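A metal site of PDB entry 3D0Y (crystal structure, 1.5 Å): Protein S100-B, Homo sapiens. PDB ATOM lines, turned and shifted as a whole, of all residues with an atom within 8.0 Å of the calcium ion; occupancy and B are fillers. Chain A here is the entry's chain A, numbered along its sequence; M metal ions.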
ATOM      1  N   PHE A  15      -4.615  20.751   2.245  1.00  0.00           N
ATOM      2  CA  PHE A  15      -5.108  22.119   2.089  1.00  0.00           C
ATOM      3  C   PHE A  15      -4.001  23.144   2.327  1.00  0.00           C
ATOM      4  O   PHE A  15      -3.761  24.017   1.490  1.00  0.00           O
ATOM      5  CB  PHE A  15      -6.279  22.429   3.016  1.00  0.00           C
ATOM      6  CG  PHE A  15      -6.821  23.804   2.817  1.00  0.00           C
ATOM      7  CD1 PHE A  15      -7.653  24.123   1.734  1.00  0.00           C
ATOM      8  CD2 PHE A  15      -6.489  24.807   3.735  1.00  0.00           C
ATOM      9  CE1 PHE A  15      -8.191  25.434   1.538  1.00  0.00           C
ATOM     10  CE2 PHE A  15      -6.995  26.089   3.582  1.00  0.00           C
ATOM     11  CZ  PHE A  15      -7.852  26.414   2.460  1.00  0.00           C
ATOM     12  N   HIS A  16      -3.345  23.016   3.476  1.00  0.00           N
ATOM     13  CA  HIS A  16      -2.301  23.963   3.825  1.00  0.00           C
ATOM     14  C   HIS A  16      -1.120  23.967   2.894  1.00  0.00           C
ATOM     15  O   HIS A  16      -0.564  25.013   2.596  1.00  0.00           O
ATOM     16  CB  HIS A  16      -1.803  23.659   5.218  1.00  0.00           C
ATOM     17  CG  HIS A  16      -2.650  24.209   6.310  1.00  0.00           C
ATOM     18  ND1 HIS A  16      -2.743  23.604   7.556  1.00  0.00           N
ATOM     19  CD2 HIS A  16      -3.445  25.311   6.367  1.00  0.00           C
ATOM     20  CE1 HIS A  16      -3.563  24.316   8.321  1.00  0.00           C
ATOM     21  NE2 HIS A  16      -4.006  25.345   7.619  1.00  0.00           N
ATOM     22  N   TYR A  18      -1.054  23.501  -0.219  1.00  0.00           N
ATOM     23  CA  TYR A  18      -1.343  24.260  -1.422  1.00  0.00           C
ATOM     24  C   TYR A  18      -1.798  25.670  -1.172  1.00  0.00           C
ATOM     25  O   TYR A  18      -1.419  26.553  -1.925  1.00  0.00           O
ATOM     26  CB  TYR A  18      -2.327  23.492  -2.270  1.00  0.00           C
ATOM     27  CG  TYR A  18      -1.637  22.334  -2.896  1.00  0.00           C
ATOM     28  CD1 TYR A  18      -1.563  21.122  -2.228  1.00  0.00           C
ATOM     29  CD2 TYR A  18      -1.001  22.466  -4.127  1.00  0.00           C
ATOM     30  CE1 TYR A  18      -0.839  20.033  -2.773  1.00  0.00           C
ATOM     31  CE2 TYR A  18      -0.313  21.392  -4.685  1.00  0.00           C
ATOM     32  CZ  TYR A  18      -0.232  20.192  -4.017  1.00  0.00           C
ATOM     33  OH  TYR A  18       0.467  19.161  -4.609  1.00  0.00           O
ATOM     34  N   SER A  19      -2.560  25.897  -0.101  1.00  0.00           N
ATOM     35  CA  SER A  19      -3.074  27.252   0.129  1.00  0.00           C
ATOM     36  C   SER A  19      -1.971  28.271   0.497  1.00  0.00           C
ATOM     37  O   SER A  19      -2.104  29.455   0.235  1.00  0.00           O
ATOM     38  CB  SER A  19      -4.152  27.228   1.223  1.00  0.00           C
ATOM     39  OG  SER A  19      -3.563  26.815   2.453  1.00  0.00           O
ATOM     40  N   GLY A  20      -0.919  27.795   1.142  1.00  0.00           N
ATOM     41  CA  GLY A  20       0.103  28.691   1.676  1.00  0.00           C
ATOM     42  C   GLY A  20       1.149  29.117   0.676  1.00  0.00           C
ATOM     43  O   GLY A  20       2.088  29.843   1.016  1.00  0.00           O
ATOM     44  N   ARG A  21       1.029  28.631  -0.555  1.00  0.00           N
ATOM     45  CA  ARG A  21       2.059  28.879  -1.547  1.00  0.00           C
ATOM     46  C   ARG A  21       2.123  30.350  -1.914  1.00  0.00           C
ATOM     47  O   ARG A  21       3.182  30.953  -1.875  1.00  0.00           O
ATOM     48  CB  ARG A  21       1.835  28.031  -2.783  1.00  0.00           C
ATOM     49  CG  ARG A  21       2.002  26.545  -2.521  1.00  0.00           C
ATOM     50  CD  ARG A  21       1.681  25.765  -3.776  1.00  0.00           C
ATOM     51  NE  ARG A  21       2.138  24.385  -3.664  1.00  0.00           N
ATOM     52  CZ  ARG A  21       2.330  23.566  -4.706  1.00  0.00           C
ATOM     53  NH1 ARG A  21       2.098  23.978  -5.936  1.00  0.00           N
ATOM     54  NH2 ARG A  21       2.737  22.313  -4.515  1.00  0.00           N
ATOM     55  N   GLU A  22       0.980  30.918  -2.258  1.00  0.00           N
ATOM     56  CA  GLU A  22       0.904  32.287  -2.660  1.00  0.00           C
ATOM     57  C   GLU A  22      -0.371  32.943  -2.118  1.00  0.00           C
ATOM     58  O   GLU A  22      -1.371  32.254  -1.738  1.00  0.00           O
ATOM     59  CB  GLU A  22       0.964  32.368  -4.176  1.00  0.00           C
ATOM     60  CG  GLU A  22       2.384  32.488  -4.699  1.00  0.00           C
ATOM     61  CD  GLU A  22       2.532  32.057  -6.154  1.00  0.00           C
ATOM     62  OE1 GLU A  22       3.595  32.376  -6.737  1.00  0.00           O
ATOM     63  OE2 GLU A  22       1.621  31.404  -6.701  1.00  0.00           O
ATOM     64  N   GLY A  23      -0.290  34.278  -2.100  1.00  0.00           N
ATOM     65  CA  GLY A  23      -1.335  35.165  -1.652  1.00  0.00           C
ATOM     66  C   GLY A  23      -1.803  34.801  -0.274  1.00  0.00           C
ATOM     67  O   GLY A  23      -0.979  34.583   0.638  1.00  0.00           O
ATOM     68  N   ASP A  24      -3.123  34.734  -0.143  1.00  0.00           N
ATOM     69  CA  ASP A  24      -3.786  34.290   1.054  1.00  0.00           C
ATOM     70  C   ASP A  24      -3.314  32.858   1.346  1.00  0.00           C
ATOM     71  O   ASP A  24      -3.451  31.947   0.521  1.00  0.00           O
ATOM     72  CB  ASP A  24      -5.296  34.319   0.838  1.00  0.00           C
ATOM     73  CG  ASP A  24      -6.097  34.231   2.126  1.00  0.00           C
ATOM     74  OD1 ASP A  24      -5.776  33.442   3.056  1.00  0.00           O
ATOM     75  OD2 ASP A  24      -7.111  34.933   2.185  1.00  0.00           O
ATOM     76  N   LYS A  25      -2.730  32.705   2.526  1.00  0.00           N
ATOM     77  CA  LYS A  25      -2.147  31.438   2.972  1.00  0.00           C
ATOM     78  C   LYS A  25      -3.220  30.419   3.360  1.00  0.00           C
ATOM     79  O   LYS A  25      -2.940  29.229   3.536  1.00  0.00           O
ATOM     80  CB  LYS A  25      -1.208  31.684   4.142  1.00  0.00           C
ATOM     81  N   HIS A  26      -4.455  30.917   3.496  1.00  0.00           N
ATOM     82  CA  HIS A  26      -5.567  30.131   3.971  1.00  0.00           C
ATOM     83  C   HIS A  26      -6.614  29.934   2.899  1.00  0.00           C
ATOM     84  O   HIS A  26      -7.694  29.397   3.150  1.00  0.00           O
ATOM     85  CB  HIS A  26      -6.157  30.802   5.201  1.00  0.00           C
ATOM     86  CG  HIS A  26      -6.189  29.898   6.384  1.00  0.00           C
ATOM     87  ND1 HIS A  26      -6.982  30.140   7.486  1.00  0.00           N
ATOM     88  CD2 HIS A  26      -5.553  28.719   6.623  1.00  0.00           C
ATOM     89  CE1 HIS A  26      -6.810  29.158   8.355  1.00  0.00           C
ATOM     90  NE2 HIS A  26      -5.957  28.284   7.859  1.00  0.00           N
ATOM     91  N   LYS A  27      -6.277  30.347   1.673  1.00  0.00           N
ATOM     92  CA  LYS A  27      -7.120  30.121   0.524  1.00  0.00           C
ATOM     93  C   LYS A  27      -6.313  29.577  -0.658  1.00  0.00           C
ATOM     94  O   LYS A  27      -5.120  29.906  -0.836  1.00  0.00           O
ATOM     95  CB  LYS A  27      -7.814  31.436   0.119  1.00  0.00           C
ATOM     96  CG  LYS A  27      -8.830  31.937   1.136  1.00  0.00           C
ATOM     97  CD  LYS A  27      -9.601  33.106   0.599  1.00  0.00           C
ATOM     98  CE  LYS A  27     -10.360  33.814   1.743  1.00  0.00           C
ATOM     99  NZ  LYS A  27      -9.498  34.065   2.948  1.00  0.00           N
ATOM    100  N   LEU A  28      -6.991  28.734  -1.437  1.00  0.00           N
ATOM    101  CA  LEU A  28      -6.535  28.276  -2.737  1.00  0.00           C
ATOM    102  C   LEU A  28      -6.935  29.277  -3.825  1.00  0.00           C
ATOM    103  O   LEU A  28      -8.113  29.523  -4.008  1.00  0.00           O
ATOM    104  CB  LEU A  28      -7.137  26.877  -3.042  1.00  0.00           C
ATOM    105  CG  LEU A  28      -6.751  25.684  -2.130  1.00  0.00           C
ATOM    106  CD1 LEU A  28      -7.618  24.452  -2.376  1.00  0.00           C
ATOM    107  CD2 LEU A  28      -5.248  25.354  -2.213  1.00  0.00           C
ATOM    108  N   LYS A  29      -5.958  29.822  -4.546  1.00  0.00           N
ATOM    109  CA  LYS A  29      -6.184  30.560  -5.776  1.00  0.00           C
ATOM    110  C   LYS A  29      -6.234  29.518  -6.891  1.00  0.00           C
ATOM    111  O   LYS A  29      -5.919  28.343  -6.641  1.00  0.00           O
ATOM    112  CB  LYS A  29      -5.060  31.588  -6.002  1.00  0.00           C
ATOM    113  N   LYS A  30      -6.653  29.917  -8.087  1.00  0.00           N
ATOM    114  CA  LYS A  30      -6.818  28.990  -9.214  1.00  0.00           C
ATOM    115  C   LYS A  30      -5.576  28.131  -9.489  1.00  0.00           C
ATOM    116  O   LYS A  30      -5.666  26.919  -9.718  1.00  0.00           O
ATOM    117  CB  LYS A  30      -7.198  29.740 -10.496  1.00  0.00           C
ATOM    118  CG  LYS A  30      -8.626  30.224 -10.563  1.00  0.00           C
ATOM    119  CD  LYS A  30      -8.870  30.809 -11.932  1.00  0.00           C
ATOM    120  CE  LYS A  30     -10.248  31.340 -12.087  1.00  0.00           C
ATOM    121  NZ  LYS A  30     -10.381  31.837 -13.455  1.00  0.00           N
ATOM    122  N   SER A  31      -4.406  28.751  -9.449  1.00  0.00           N
ATOM    123  CA  SER A  31      -3.181  27.984  -9.687  1.00  0.00           C
ATOM    124  C   SER A  31      -2.853  26.975  -8.569  1.00  0.00           C
ATOM    125  O   SER A  31      -2.394  25.848  -8.835  1.00  0.00           O
ATOM    126  CB  SER A  31      -2.008  28.924  -9.911  1.00  0.00           C
ATOM    127  OG  SER A  31      -1.726  29.615  -8.713  1.00  0.00           O
ATOM    128  N   GLU A  32      -3.120  27.373  -7.322  1.00  0.00           N
ATOM    129  CA  GLU A  32      -2.999  26.461  -6.180  1.00  0.00           C
ATOM    130  C   GLU A  32      -3.955  25.284  -6.283  1.00  0.00           C
ATOM    131  O   GLU A  32      -3.613  24.128  -5.976  1.00  0.00           O
ATOM    132  CB  GLU A  32      -3.212  27.215  -4.881  1.00  0.00           C
ATOM    133  CG  GLU A  32      -2.026  28.094  -4.551  1.00  0.00           C
ATOM    134  CD  GLU A  32      -2.329  29.058  -3.432  1.00  0.00           C
ATOM    135  OE1 GLU A  32      -3.520  29.332  -3.183  1.00  0.00           O
ATOM    136  OE2 GLU A  32      -1.364  29.566  -2.796  1.00  0.00           O
ATOM    137  N   LEU A  33      -5.184  25.571  -6.692  1.00  0.00           N
ATOM    138  CA  LEU A  33      -6.199  24.530  -6.826  1.00  0.00           C
ATOM    139  C   LEU A  33      -5.843  23.578  -7.984  1.00  0.00           C
ATOM    140  O   LEU A  33      -5.936  22.357  -7.840  1.00  0.00           O
ATOM    141  CB  LEU A  33      -7.546  25.201  -7.017  1.00  0.00           C
ATOM    142  CG  LEU A  33      -8.738  24.280  -7.270  1.00  0.00           C
ATOM    143  CD1 LEU A  33      -9.038  23.420  -6.069  1.00  0.00           C
ATOM    144  CD2 LEU A  33      -9.919  25.127  -7.619  1.00  0.00           C
ATOM    145  N   GLU A  68     -11.576  32.471  -4.762  1.00  0.00           N
ATOM    146  CA  GLU A  68     -10.655  31.539  -4.134  1.00  0.00           C
ATOM    147  C   GLU A  68     -11.437  30.481  -3.405  1.00  0.00           C
ATOM    148  O   GLU A  68     -12.631  30.673  -3.117  1.00  0.00           O
ATOM    149  CB  GLU A  68      -9.738  32.210  -3.094  1.00  0.00           C
ATOM    150  CG  GLU A  68      -9.161  33.511  -3.539  1.00  0.00           C
ATOM    151  CD  GLU A  68      -7.647  33.579  -3.514  1.00  0.00           C
ATOM    152  OE1 GLU A  68      -6.994  32.858  -2.718  1.00  0.00           O
ATOM    153  OE2 GLU A  68      -7.090  34.368  -4.309  1.00  0.00           O
ATOM    154  N   CYS A  69     -10.745  29.378  -3.121  1.00  0.00           N
ATOM    155  CA  CYS A  69     -11.320  28.269  -2.372  1.00  0.00           C
ATOM    156  C   CYS A  69     -10.797  28.288  -0.955  1.00  0.00           C
ATOM    157  O   CYS A  69      -9.599  28.064  -0.730  1.00  0.00           O
ATOM    158  CB  CYS A  69     -10.981  26.934  -3.030  1.00  0.00           C
ATOM    159  SG  CYS A  69     -11.713  25.516  -2.206  1.00  0.00           S
HETATM  160 CA    CA M   1      -3.037  30.803  -1.395  1.00  0.00          CA
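The calcium ion is bound by O of Glu 22 (2.2 Å), O of Asp 24 (2.3 Å), O of Ser 19 (2.3 Å), O of Lys 27 (2.3 Å), OE1 of Glu 32 (2.4 Å) and OE2 of Glu 32 (2.5 Å). The calcium ion has six donor atoms within binding distance.
The side-chain carboxylate of Asp 24 sits at hydrogen-bond distance from the backbone NH of His 26. The backbone carbonyl oxygen (O) of Lys 25 lies within hydrogen-bond range of the side-chain hydroxyl (OG) of Ser 19, at 2.7 Å. The side-chain carboxylate of Glu 32 sits close to the backbone NH of Arg 21 (3.4 Å). The side-chain amino group (NZ) of Lys 27 is in salt-bridge range of the side-chain carboxylate (OD2) of Asp 24 (2.7 Å). The side-chain carboxylate (OE1) of Glu 32 sits close to the backbone NH (N) of Lys 29. The backbone carbonyl oxygen of Phe 15 sits at hydrogen-bond distance from the side-chain hydroxyl of Ser 19 (3.0 Å).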
